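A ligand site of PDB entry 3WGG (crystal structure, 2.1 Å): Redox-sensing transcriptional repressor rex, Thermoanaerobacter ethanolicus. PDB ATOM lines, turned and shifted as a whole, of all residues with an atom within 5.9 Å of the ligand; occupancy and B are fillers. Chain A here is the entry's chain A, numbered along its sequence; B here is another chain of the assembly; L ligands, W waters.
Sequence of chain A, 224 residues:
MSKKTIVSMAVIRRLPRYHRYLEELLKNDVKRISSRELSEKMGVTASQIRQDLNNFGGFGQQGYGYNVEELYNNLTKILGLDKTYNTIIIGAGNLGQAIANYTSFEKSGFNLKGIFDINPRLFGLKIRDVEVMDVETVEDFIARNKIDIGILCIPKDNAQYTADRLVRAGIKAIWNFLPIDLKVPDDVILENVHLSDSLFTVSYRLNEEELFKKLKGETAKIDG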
ATOM      1  N   ILE A  90      -2.712   3.897  -2.893  1.00  0.00           N
ATOM      2  CA  ILE A  90      -2.380   3.794  -1.481  1.00  0.00           C
ATOM      3  C   ILE A  90      -2.687   2.371  -1.068  1.00  0.00           C
ATOM      4  O   ILE A  90      -3.815   1.910  -1.245  1.00  0.00           O
ATOM      5  CB  ILE A  90      -3.190   4.773  -0.614  1.00  0.00           C
ATOM      6  CG1 ILE A  90      -3.417   6.109  -1.328  1.00  0.00           C
ATOM      7  CG2 ILE A  90      -2.548   4.908   0.752  1.00  0.00           C
ATOM      8  CD1 ILE A  90      -2.179   6.918  -1.620  1.00  0.00           C
ATOM      9  N   GLY A  91      -1.679   1.692  -0.528  1.00  0.00           N
ATOM     10  CA  GLY A  91      -1.728   0.295  -0.088  1.00  0.00           C
ATOM     11  C   GLY A  91      -0.927  -0.505  -1.090  1.00  0.00           C
ATOM     12  O   GLY A  91      -1.342  -0.652  -2.247  1.00  0.00           O
ATOM     13  N   ALA A  92       0.213  -1.021  -0.680  1.00  0.00           N
ATOM     14  CA  ALA A  92       1.002  -1.887  -1.539  1.00  0.00           C
ATOM     15  C   ALA A  92       0.946  -3.329  -1.078  1.00  0.00           C
ATOM     16  O   ALA A  92       1.946  -4.026  -1.093  1.00  0.00           O
ATOM     17  CB  ALA A  92       2.464  -1.407  -1.600  1.00  0.00           C
ATOM     18  N   GLY A  93      -0.213  -3.793  -0.642  1.00  0.00           N
ATOM     19  CA  GLY A  93      -0.354  -5.219  -0.320  1.00  0.00           C
ATOM     20  C   GLY A  93      -0.737  -5.904  -1.617  1.00  0.00           C
ATOM     21  O   GLY A  93      -0.456  -5.393  -2.698  1.00  0.00           O
ATOM     22  N   ASN A  94      -1.332  -7.093  -1.545  1.00  0.00           N
ATOM     23  CA  ASN A  94      -1.635  -7.791  -2.776  1.00  0.00           C
ATOM     24  C   ASN A  94      -2.565  -7.033  -3.728  1.00  0.00           C
ATOM     25  O   ASN A  94      -2.376  -7.065  -4.908  1.00  0.00           O
ATOM     26  CB  ASN A  94      -2.265  -9.143  -2.449  1.00  0.00           C
ATOM     27  CG  ASN A  94      -1.298 -10.066  -1.767  1.00  0.00           C
ATOM     28  OD1 ASN A  94      -1.584 -10.547  -0.695  1.00  0.00           O
ATOM     29  ND2 ASN A  94      -0.152 -10.292  -2.370  1.00  0.00           N
ATOM     30  N   LEU A  95      -3.589  -6.380  -3.212  1.00  0.00           N
ATOM     31  CA  LEU A  95      -4.491  -5.668  -4.078  1.00  0.00           C
ATOM     32  C   LEU A  95      -3.790  -4.495  -4.740  1.00  0.00           C
ATOM     33  O   LEU A  95      -3.885  -4.335  -5.951  1.00  0.00           O
ATOM     34  CB  LEU A  95      -5.738  -5.207  -3.327  1.00  0.00           C
ATOM     35  CG  LEU A  95      -6.748  -4.394  -4.151  1.00  0.00           C
ATOM     36  CD1 LEU A  95      -7.303  -5.200  -5.284  1.00  0.00           C
ATOM     37  CD2 LEU A  95      -7.857  -3.889  -3.230  1.00  0.00           C
ATOM     38  N   GLY A  96      -3.111  -3.640  -3.974  1.00  0.00           N
ATOM     39  CA  GLY A  96      -2.511  -2.473  -4.584  1.00  0.00           C
ATOM     40  C   GLY A  96      -1.454  -2.891  -5.603  1.00  0.00           C
ATOM     41  O   GLY A  96      -1.304  -2.242  -6.604  1.00  0.00           O
ATOM     42  N   PHE A 116       2.053   4.075  -2.091  1.00  0.00           N
ATOM     43  CA  PHE A 116       2.287   4.430  -0.714  1.00  0.00           C
ATOM     44  C   PHE A 116       1.822   3.358   0.258  1.00  0.00           C
ATOM     45  O   PHE A 116       0.805   2.676   0.020  1.00  0.00           O
ATOM     46  CB  PHE A 116       1.625   5.775  -0.396  1.00  0.00           C
ATOM     47  CG  PHE A 116       2.146   6.874  -1.229  1.00  0.00           C
ATOM     48  CD1 PHE A 116       3.187   7.677  -0.766  1.00  0.00           C
ATOM     49  CD2 PHE A 116       1.655   7.086  -2.509  1.00  0.00           C
ATOM     50  CE1 PHE A 116       3.703   8.677  -1.583  1.00  0.00           C
ATOM     51  CE2 PHE A 116       2.183   8.080  -3.330  1.00  0.00           C
ATOM     52  CZ  PHE A 116       3.179   8.887  -2.855  1.00  0.00           C
ATOM     53  N   ASP A 117       2.577   3.184   1.335  1.00  0.00           N
ATOM     54  CA  ASP A 117       2.192   2.241   2.370  1.00  0.00           C
ATOM     55  C   ASP A 117       2.606   2.727   3.735  1.00  0.00           C
ATOM     56  O   ASP A 117       3.383   3.663   3.842  1.00  0.00           O
ATOM     57  CB  ASP A 117       2.772   0.875   2.087  1.00  0.00           C
ATOM     58  CG  ASP A 117       1.924  -0.238   2.670  1.00  0.00           C
ATOM     59  OD1 ASP A 117       1.164  -0.834   1.882  1.00  0.00           O
ATOM     60  OD2 ASP A 117       1.980  -0.524   3.890  1.00  0.00           O
ATOM     61  N   ILE A 118       2.086   2.065   4.774  1.00  0.00           N
ATOM     62  CA  ILE A 118       2.497   2.310   6.143  1.00  0.00           C
ATOM     63  C   ILE A 118       3.571   1.323   6.610  1.00  0.00           C
ATOM     64  O   ILE A 118       4.305   1.617   7.550  1.00  0.00           O
ATOM     65  CB  ILE A 118       1.339   2.235   7.162  1.00  0.00           C
ATOM     66  CG1 ILE A 118       0.499   0.958   6.986  1.00  0.00           C
ATOM     67  CG2 ILE A 118       0.489   3.437   7.094  1.00  0.00           C
ATOM     68  CD1 ILE A 118      -0.208   0.556   8.242  1.00  0.00           C
ATOM     69  N   ASN A 119       3.626   0.172   5.955  1.00  0.00           N
ATOM     70  CA  ASN A 119       4.562  -0.897   6.302  1.00  0.00           C
ATOM     71  C   ASN A 119       6.010  -0.567   5.910  1.00  0.00           C
ATOM     72  O   ASN A 119       6.357  -0.609   4.710  1.00  0.00           O
ATOM     73  CB  ASN A 119       4.140  -2.213   5.610  1.00  0.00           C
ATOM     74  CG  ASN A 119       4.930  -3.430   6.092  1.00  0.00           C
ATOM     75  OD1 ASN A 119       5.910  -3.290   6.838  1.00  0.00           O
ATOM     76  ND2 ASN A 119       4.515  -4.626   5.671  1.00  0.00           N
ATOM     77  N   LEU A 122       8.110  -2.463   3.410  1.00  0.00           N
ATOM     78  CA  LEU A 122       7.782  -2.328   1.983  1.00  0.00           C
ATOM     79  C   LEU A 122       8.420  -1.097   1.401  1.00  0.00           C
ATOM     80  O   LEU A 122       8.453  -0.993   0.181  1.00  0.00           O
ATOM     81  CB  LEU A 122       6.253  -2.235   1.738  1.00  0.00           C
ATOM     82  CG  LEU A 122       5.459  -3.493   2.082  1.00  0.00           C
ATOM     83  CD1 LEU A 122       3.944  -3.267   1.902  1.00  0.00           C
ATOM     84  CD2 LEU A 122       5.964  -4.744   1.321  1.00  0.00           C
ATOM     85  N   VAL A 135       3.526   6.525   3.329  1.00  0.00           N
ATOM     86  CA  VAL A 135       2.348   7.306   2.992  1.00  0.00           C
ATOM     87  C   VAL A 135       2.370   8.614   3.788  1.00  0.00           C
ATOM     88  O   VAL A 135       1.554   9.532   3.582  1.00  0.00           O
ATOM     89  CB  VAL A 135       1.036   6.488   3.284  1.00  0.00           C
ATOM     90  CG1 VAL A 135       0.948   6.082   4.774  1.00  0.00           C
ATOM     91  CG2 VAL A 135      -0.191   7.247   2.837  1.00  0.00           C
ATOM     92  N   CYS A 153      -6.380   1.084  -1.827  1.00  0.00           N
ATOM     93  CA  CYS A 153      -6.258  -0.375  -1.742  1.00  0.00           C
ATOM     94  C   CYS A 153      -5.796  -0.782  -0.333  1.00  0.00           C
ATOM     95  O   CYS A 153      -4.955  -1.689  -0.123  1.00  0.00           O
ATOM     96  CB  CYS A 153      -5.294  -0.881  -2.806  1.00  0.00           C
ATOM     97  SG  CYS A 153      -5.766  -0.454  -4.512  1.00  0.00           S
ATOM     98  N   ILE A 154      -6.372  -0.074   0.649  1.00  0.00           N
ATOM     99  CA  ILE A 154      -6.041  -0.276   2.050  1.00  0.00           C
ATOM    100  C   ILE A 154      -7.194  -0.934   2.801  1.00  0.00           C
ATOM    101  O   ILE A 154      -8.277  -0.998   2.263  1.00  0.00           O
ATOM    102  CB  ILE A 154      -5.696   1.039   2.741  1.00  0.00           C
ATOM    103  CG1 ILE A 154      -6.869   2.031   2.631  1.00  0.00           C
ATOM    104  CG2 ILE A 154      -4.391   1.596   2.180  1.00  0.00           C
ATOM    105  CD1 ILE A 154      -6.790   3.179   3.549  1.00  0.00           C
ATOM    106  N   PRO A 155      -6.947  -1.396   4.054  1.00  0.00           N
ATOM    107  CA  PRO A 155      -8.052  -1.964   4.842  1.00  0.00           C
ATOM    108  C   PRO A 155      -9.040  -0.863   5.218  1.00  0.00           C
ATOM    109  O   PRO A 155      -8.704   0.319   5.198  1.00  0.00           O
ATOM    110  CB  PRO A 155      -7.341  -2.566   6.094  1.00  0.00           C
ATOM    111  CG  PRO A 155      -5.846  -2.650   5.727  1.00  0.00           C
ATOM    112  CD  PRO A 155      -5.638  -1.517   4.719  1.00  0.00           C
ATOM    113  N   LYS A 156     -10.280  -1.262   5.457  1.00  0.00           N
ATOM    114  CA  LYS A 156     -11.398  -0.343   5.661  1.00  0.00           C
ATOM    115  C   LYS A 156     -11.166   0.662   6.785  1.00  0.00           C
ATOM    116  O   LYS A 156     -11.528   1.820   6.689  1.00  0.00           O
ATOM    117  CB  LYS A 156     -12.628  -1.119   6.134  1.00  0.00           C
ATOM    118  CG  LYS A 156     -13.400  -1.875   5.117  1.00  0.00           C
ATOM    119  CD  LYS A 156     -14.539  -2.619   5.830  1.00  0.00           C
ATOM    120  CE  LYS A 156     -13.999  -3.787   6.658  1.00  0.00           C
ATOM    121  NZ  LYS A 156     -14.450  -3.711   8.082  1.00  0.00           N
ATOM    122  N   ASP A 157     -10.608   0.165   7.883  1.00  0.00           N
ATOM    123  CA  ASP A 157     -10.735   0.836   9.168  1.00  0.00           C
ATOM    124  C   ASP A 157     -10.228   2.283   9.204  1.00  0.00           C
ATOM    125  O   ASP A 157     -10.569   3.062  10.101  1.00  0.00           O
ATOM    126  CB  ASP A 157      -9.967   0.006  10.198  1.00  0.00           C
ATOM    127  CG  ASP A 157      -8.598  -0.367   9.685  1.00  0.00           C
ATOM    128  OD1 ASP A 157      -7.990   0.517   9.040  1.00  0.00           O
ATOM    129  OD2 ASP A 157      -8.148  -1.519   9.883  1.00  0.00           O
ATOM    130  N   ASN A 158      -9.429   2.654   8.211  1.00  0.00           N
ATOM    131  CA  ASN A 158      -8.773   3.966   8.228  1.00  0.00           C
ATOM    132  C   ASN A 158      -8.694   4.507   6.805  1.00  0.00           C
ATOM    133  O   ASN A 158      -7.855   5.371   6.493  1.00  0.00           O
ATOM    134  CB  ASN A 158      -7.376   3.832   8.831  1.00  0.00           C
ATOM    135  CG  ASN A 158      -6.463   2.912   7.990  1.00  0.00           C
ATOM    136  OD1 ASN A 158      -6.703   2.705   6.796  1.00  0.00           O
ATOM    137  ND2 ASN A 158      -5.432   2.351   8.632  1.00  0.00           N
ATOM    138  N   THR A 162      -7.522   8.482   5.486  1.00  0.00           N
ATOM    139  CA  THR A 162      -6.637   8.567   4.336  1.00  0.00           C
ATOM    140  C   THR A 162      -7.299   9.332   3.191  1.00  0.00           C
ATOM    141  O   THR A 162      -6.673  10.166   2.528  1.00  0.00           O
ATOM    142  CB  THR A 162      -6.171   7.139   3.925  1.00  0.00           C
ATOM    143  OG1 THR A 162      -5.120   6.741   4.791  1.00  0.00           O
ATOM    144  CG2 THR A 162      -5.683   7.101   2.500  1.00  0.00           C
ATOM    145  N   PHE A 177     -11.428   0.948  -3.679  1.00  0.00           N
ATOM    146  CA  PHE A 177     -11.702  -0.513  -3.655  1.00  0.00           C
ATOM    147  C   PHE A 177     -12.354  -1.032  -2.379  1.00  0.00           C
ATOM    148  O   PHE A 177     -12.786  -2.186  -2.335  1.00  0.00           O
ATOM    149  CB  PHE A 177     -10.471  -1.356  -4.019  1.00  0.00           C
ATOM    150  CG  PHE A 177     -10.165  -1.369  -5.501  1.00  0.00           C
ATOM    151  CD1 PHE A 177     -10.535  -2.431  -6.283  1.00  0.00           C
ATOM    152  CD2 PHE A 177      -9.541  -0.277  -6.098  1.00  0.00           C
ATOM    153  CE1 PHE A 177     -10.258  -2.465  -7.641  1.00  0.00           C
ATOM    154  CE2 PHE A 177      -9.263  -0.278  -7.456  1.00  0.00           C
ATOM    155  CZ  PHE A 177      -9.640  -1.410  -8.244  1.00  0.00           C
ATOM    156  N   LEU A 178     -12.486  -0.172  -1.357  1.00  0.00           N
ATOM    157  CA  LEU A 178     -13.072  -0.595  -0.070  1.00  0.00           C
ATOM    158  C   LEU A 178     -14.604  -0.512   0.023  1.00  0.00           C
ATOM    159  O   LEU A 178     -15.210   0.444  -0.475  1.00  0.00           O
ATOM    160  CB  LEU A 178     -12.436   0.153   1.108  1.00  0.00           C
ATOM    161  CG  LEU A 178     -11.086   0.874   0.976  1.00  0.00           C
ATOM    162  CD1 LEU A 178     -10.597   1.228   2.344  1.00  0.00           C
ATOM    163  CD2 LEU A 178     -10.032   0.090   0.231  1.00  0.00           C
ATOM    164  N   PRO A 179     -15.252  -1.520   0.677  1.00  0.00           N
ATOM    165  CA  PRO A 179     -16.706  -1.425   0.878  1.00  0.00           C
ATOM    166  C   PRO A 179     -17.023  -0.611   2.117  1.00  0.00           C
ATOM    167  O   PRO A 179     -17.503  -1.151   3.110  1.00  0.00           O
ATOM    168  CB  PRO A 179     -17.105  -2.877   1.087  1.00  0.00           C
ATOM    169  CG  PRO A 179     -15.950  -3.451   1.818  1.00  0.00           C
ATOM    170  CD  PRO A 179     -14.710  -2.772   1.227  1.00  0.00           C
ATOM    171  N   GLN B  97      -4.221 -13.684  -4.753  1.00  0.00           N
ATOM    172  CA  GLN B  97      -4.218 -13.550  -3.286  1.00  0.00           C
ATOM    173  C   GLN B  97      -5.147 -12.428  -2.856  1.00  0.00           C
ATOM    174  O   GLN B  97      -5.835 -12.564  -1.847  1.00  0.00           O
ATOM    175  CB  GLN B  97      -2.812 -13.276  -2.792  1.00  0.00           C
ATOM    176  CG  GLN B  97      -1.922 -14.507  -2.961  1.00  0.00           C
ATOM    177  CD  GLN B  97      -0.504 -14.340  -2.397  1.00  0.00           C
ATOM    178  OE1 GLN B  97      -0.320 -13.841  -1.314  1.00  0.00           O
ATOM    179  NE2 GLN B  97       0.489 -14.770  -3.162  1.00  0.00           N
ATOM    180  N   ALA B  98      -5.136 -11.298  -3.592  1.00  0.00           N
ATOM    181  CA  ALA B  98      -6.099 -10.260  -3.196  1.00  0.00           C
ATOM    182  C   ALA B  98      -7.522 -10.826  -3.175  1.00  0.00           C
ATOM    183  O   ALA B  98      -8.278 -10.563  -2.260  1.00  0.00           O
ATOM    184  CB  ALA B  98      -5.976  -9.012  -4.108  1.00  0.00           C
ATOM    185  N   ASN B 101      -8.466 -12.995  -0.484  1.00  0.00           N
ATOM    186  CA  ASN B 101      -8.713 -12.139   0.659  1.00  0.00           C
ATOM    187  C   ASN B 101     -10.066 -11.387   0.663  1.00  0.00           C
ATOM    188  O   ASN B 101     -10.360 -10.668   1.628  1.00  0.00           O
ATOM    189  CB  ASN B 101      -7.543 -11.149   0.811  1.00  0.00           C
ATOM    190  CG  ASN B 101      -7.527 -10.478   2.131  1.00  0.00           C
ATOM    191  OD1 ASN B 101      -8.071 -11.005   3.097  1.00  0.00           O
ATOM    192  ND2 ASN B 101      -6.924  -9.293   2.191  1.00  0.00           N
ATOM    193  N   TYR B 102     -10.883 -11.509  -0.377  1.00  0.00           N
ATOM    194  CA  TYR B 102     -12.261 -10.986  -0.271  1.00  0.00           C
ATOM    195  C   TYR B 102     -13.109 -11.879   0.638  1.00  0.00           C
ATOM    196  O   TYR B 102     -13.941 -12.670   0.164  1.00  0.00           O
ATOM    197  CB  TYR B 102     -12.901 -10.793  -1.637  1.00  0.00           C
ATOM    198  CG  TYR B 102     -12.600  -9.436  -2.244  1.00  0.00           C
ATOM    199  CD1 TYR B 102     -13.635  -8.554  -2.621  1.00  0.00           C
ATOM    200  CD2 TYR B 102     -11.292  -9.019  -2.384  1.00  0.00           C
ATOM    201  CE1 TYR B 102     -13.313  -7.281  -3.171  1.00  0.00           C
ATOM    202  CE2 TYR B 102     -10.981  -7.770  -2.907  1.00  0.00           C
ATOM    203  CZ  TYR B 102     -11.972  -6.913  -3.289  1.00  0.00           C
ATOM    204  OH  TYR B 102     -11.579  -5.693  -3.803  1.00  0.00           O
ATOM    205  N   THR B 103     -12.870 -11.803   1.942  1.00  0.00           N
ATOM    206  CA  THR B 103     -13.441 -12.773   2.855  1.00  0.00           C
ATOM    207  C   THR B 103     -14.940 -12.569   3.031  1.00  0.00           C
ATOM    208  O   THR B 103     -15.655 -13.493   3.412  1.00  0.00           O
ATOM    209  CB  THR B 103     -12.735 -12.730   4.229  1.00  0.00           C
ATOM    210  OG1 THR B 103     -12.722 -11.374   4.690  1.00  0.00           O
ATOM    211  CG2 THR B 103     -11.294 -13.224   4.135  1.00  0.00           C
ATOM    212  N   SER B 104     -15.461 -11.380   2.739  1.00  0.00           N
ATOM    213  CA  SER B 104     -16.915 -11.208   2.838  1.00  0.00           C
ATOM    214  C   SER B 104     -17.643 -12.247   1.972  1.00  0.00           C
ATOM    215  O   SER B 104     -18.704 -12.721   2.327  1.00  0.00           O
ATOM    216  CB  SER B 104     -17.341  -9.767   2.479  1.00  0.00           C
ATOM    217  OG  SER B 104     -17.507  -9.548   1.080  1.00  0.00           O
ATOM    218  N   PHE B 105     -17.069 -12.665   0.846  1.00  0.00           N
ATOM    219  CA  PHE B 105     -17.782 -13.632  -0.018  1.00  0.00           C
ATOM    220  C   PHE B 105     -18.158 -14.933   0.688  1.00  0.00           C
ATOM    221  O   PHE B 105     -19.205 -15.504   0.378  1.00  0.00           O
ATOM    222  CB  PHE B 105     -17.038 -13.919  -1.324  1.00  0.00           C
ATOM    223  CG  PHE B 105     -16.764 -12.686  -2.163  1.00  0.00           C
ATOM    224  CD1 PHE B 105     -17.617 -11.582  -2.107  1.00  0.00           C
ATOM    225  CD2 PHE B 105     -15.688 -12.640  -3.009  1.00  0.00           C
ATOM    226  CE1 PHE B 105     -17.349 -10.423  -2.902  1.00  0.00           C
ATOM    227  CE2 PHE B 105     -15.457 -11.523  -3.840  1.00  0.00           C
ATOM    228  CZ  PHE B 105     -16.280 -10.404  -3.771  1.00  0.00           C
ATOM    229  N   ARG B 128      -4.946 -17.855   3.585  1.00  0.00           N
ATOM    230  CA  ARG B 128      -5.949 -18.136   4.609  1.00  0.00           C
ATOM    231  C   ARG B 128      -6.018 -19.613   4.881  1.00  0.00           C
ATOM    232  O   ARG B 128      -5.107 -20.227   5.408  1.00  0.00           O
ATOM    233  CB  ARG B 128      -7.369 -17.663   4.203  1.00  0.00           C
ATOM    234  CG  ARG B 128      -7.471 -16.859   2.905  1.00  0.00           C
ATOM    235  CD  ARG B 128      -7.332 -15.366   3.114  1.00  0.00           C
ATOM    236  NE  ARG B 128      -6.500 -14.792   2.051  1.00  0.00           N
ATOM    237  CZ  ARG B 128      -5.938 -13.585   2.067  1.00  0.00           C
ATOM    238  NH1 ARG B 128      -5.173 -13.178   1.045  1.00  0.00           N
ATOM    239  NH2 ARG B 128      -6.140 -12.808   3.112  1.00  0.00           N
HETATM  240  P1  LIG L   1      -3.031  -6.596   2.338  1.00  0.00           P
HETATM  241  O1  LIG L   1      -2.986  -6.813   3.835  1.00  0.00           O
HETATM  242  O2  LIG L   1      -2.327  -7.552   1.392  1.00  0.00           O
HETATM  243  O3  LIG L   1      -2.589  -5.069   2.049  1.00  0.00           O
HETATM  244  C1  LIG L   1      -3.109  -3.929   2.738  1.00  0.00           C
HETATM  245  C2  LIG L   1      -1.934  -2.963   2.747  1.00  0.00           C
HETATM  246  O4  LIG L   1      -2.275  -1.655   3.164  1.00  0.00           O
HETATM  247  C3  LIG L   1      -0.848  -3.435   3.694  1.00  0.00           C
HETATM  248  O5  LIG L   1       0.343  -3.443   2.907  1.00  0.00           O
HETATM  249  C4  LIG L   1      -0.818  -2.355   4.791  1.00  0.00           C
HETATM  250  O6  LIG L   1       0.517  -2.095   5.236  1.00  0.00           O
HETATM  251  C5  LIG L   1      -1.269  -1.143   4.015  1.00  0.00           C
HETATM  252  N1  LIG L   1      -1.942  -0.125   4.806  1.00  0.00           N
HETATM  253  C6  LIG L   1      -2.737  -0.265   5.896  1.00  0.00           C
HETATM  254  N2  LIG L   1      -3.196   0.972   6.226  1.00  0.00           N
HETATM  255  C7  LIG L   1      -2.656   1.856   5.352  1.00  0.00           C
HETATM  256  C8  LIG L   1      -2.702   3.230   5.190  1.00  0.00           C
HETATM  257  N3  LIG L   1      -3.435   3.998   6.026  1.00  0.00           N
HETATM  258  N4  LIG L   1      -2.017   3.804   4.192  1.00  0.00           N
HETATM  259  C9  LIG L   1      -1.241   3.098   3.356  1.00  0.00           C
HETATM  260  N5  LIG L   1      -1.134   1.791   3.492  1.00  0.00           N
HETATM  261  C10 LIG L   1      -1.836   1.155   4.474  1.00  0.00           C
HETATM  262  O7  LIG L   1      -4.618  -6.602   1.918  1.00  0.00           O
HETATM  263  P2  LIG L   1      -5.052  -6.668   0.360  1.00  0.00           P
HETATM  264  O8  LIG L   1      -5.214  -8.103  -0.042  1.00  0.00           O
HETATM  265  O9  LIG L   1      -4.109  -5.836  -0.486  1.00  0.00           O
HETATM  266  O10 LIG L   1      -6.559  -6.055   0.388  1.00  0.00           O
HETATM  267  C11 LIG L   1      -6.873  -4.658   0.606  1.00  0.00           C
HETATM  268  C12 LIG L   1      -8.399  -4.472   0.719  1.00  0.00           C
HETATM  269  O11 LIG L   1      -9.082  -5.463  -0.081  1.00  0.00           O
HETATM  270  C13 LIG L   1      -8.971  -4.659   2.119  1.00  0.00           C
HETATM  271  O12 LIG L   1     -10.139  -3.812   2.257  1.00  0.00           O
HETATM  272  C14 LIG L   1      -9.457  -6.093   2.116  1.00  0.00           C
HETATM  273  O13 LIG L   1     -10.562  -6.105   2.991  1.00  0.00           O
HETATM  274  C15 LIG L   1      -9.849  -6.403   0.672  1.00  0.00           C
HETATM  275  N6  LIG L   1     -11.279  -6.149   0.305  1.00  0.00           N
HETATM  276  C16 LIG L   1     -12.244  -7.105   0.581  1.00  0.00           C
HETATM  277  C17 LIG L   1     -13.555  -6.956   0.290  1.00  0.00           C
HETATM  278  C18 LIG L   1     -14.473  -8.046   0.649  1.00  0.00           C
HETATM  279  O14 LIG L   1     -14.105  -8.945   1.410  1.00  0.00           O
HETATM  280  N7  LIG L   1     -15.680  -8.022   0.093  1.00  0.00           N
HETATM  281  C19 LIG L   1     -14.052  -5.714  -0.431  1.00  0.00           C
HETATM  282  C20 LIG L   1     -12.910  -4.762  -0.730  1.00  0.00           C
HETATM  283  C21 LIG L   1     -11.635  -4.996  -0.373  1.00  0.00           C
HETATM  284  O   HOH W   1       2.013  -5.234   4.204  1.00  0.00           O
HETATM  285  O   HOH W   2      -3.837 -10.314   0.445  1.00  0.00           O
HETATM  286  O   HOH W   3       0.929  -8.301   1.847  1.00  0.00           O
HETATM  287  O   HOH W   4       0.872  -2.843   7.899  1.00  0.00           O
HETATM  288  O   HOH W   5      -5.451  -6.307   4.906  1.00  0.00           O
HETATM  289  O   HOH W   6      -3.133  -3.477  -0.972  1.00  0.00           O
HETATM  290  O   HOH W   7     -10.990  -4.244   5.071  1.00  0.00           O
HETATM  291  O   HOH W   8     -13.320  -7.493   4.308  1.00  0.00           O
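The side-chain carboxylate (OD2) of Asp 117 sits at hydrogen-bond distance from an oxygen (O6) of the ligand, at 2.5 Å. O14 of the ligand lies within hydrogen-bond range of N of Ser 104 of chain B (3.1 Å). A nitrogen (N7) of the ligand lies within hydrogen-bond range of the side-chain hydroxyl (OG) of Ser 104 of chain B, 2.6 Å away. N of Leu 95 lies within hydrogen-bond range of O9 of the ligand (2.8 Å). The side-chain amide nitrogen (ND2) of Asn 101 of chain B lies within hydrogen-bond range of an oxygen (O8) of the ligand. An oxygen (O2) of the ligand is in hydrogen-bond range of the backbone NH (N) of Asn 94, at 3.1 Å. O14 of the ligand lies within hydrogen-bond range of N of Thr 103 of chain B (3.2 Å). An oxygen (O12) of the ligand lies within hydrogen-bond range of the backbone carbonyl oxygen (O) of Ile 154, 3.4 Å away. N of Ile 118 sits at hydrogen-bond distance from N5 of the ligand, at 3.5 Å. The side-chain hydroxyl of Thr 162 is in hydrogen-bond range of a nitrogen (N3) of the ligand, at 3.4 Å.
The side-chain carboxylate (OD2) of Asp 117 sits at hydrogen-bond distance from the backbone NH (N) of Asn 119 (2.7 Å). The backbone carbonyl oxygen (O) of Asp 117 sits at hydrogen-bond distance from the backbone NH (N) of Val 135 (2.9 Å). OD1 of Asp 117 sits at hydrogen-bond distance from N of Ala 92 (2.7 Å). The guanidinium group (NH2) of Arg 128 of chain B is in hydrogen-bond range of the side-chain amide oxygen (OD1) of Asn 101 of chain B (2.6 Å). The side-chain amide oxygen (OD1) of Asn 158 lies close to the backbone carbonyl oxygen (O) of Pro 155, 3.5 Å away. O of Ile 90 lies within hydrogen-bond range of N of Cys 153 (2.8 Å). The side-chain amide nitrogen (ND2) of Asn 158 sits close to the side-chain carboxylate (OD1) of Asp 157, 3.2 Å away. O of Phe 116 is in hydrogen-bond range of N of Gly 91 (2.7 Å).
Merely in contact with the ligand: Phe 177, Tyr 102 of chain B, Gly 93, Pro 179, Pro 155, Ile 90, Asn 158, Cys 153, Asn 119, Leu 122, Val 135, Gly 91, Ala 98 of chain B and Phe 116. Within 4 Å of the ligand: Ile 90, Gly 91, Gly 93, Asn 94, Leu 95, Phe 116, Asp 117, Ile 118, Asn 119, Leu 122, Val 135, Cys 153, Ile 154, Pro 155, Asn 158, Thr 162, Phe 177, Pro 179, Ala 98 of chain B, Asn 101 of chain B, Tyr 102 of chain B, Thr 103 of chain B and Ser 104 of chain B.
Water W6 lies within hydrogen-bond range of an oxygen (O9) of the ligand (2.6 Å), the backbone carbonyl oxygen of Cys 153 (2.7 Å), the backbone NH of Gly 93 (3.0 Å) and the backbone NH of Gly 96 (3.0 Å). Water W2 lies within hydrogen-bond range of OD1 of Asn 94 (2.5 Å), O8 of the ligand (2.6 Å) and NH1 of Arg 128 of chain B (3.2 Å). Water W1 bridges an oxygen (O5) of the ligand and the side-chain amide nitrogen (ND2) of Asn 119. Water W7 bridges O13 of the ligand (2.8 Å) and N of Lys 156 (3.1 Å).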
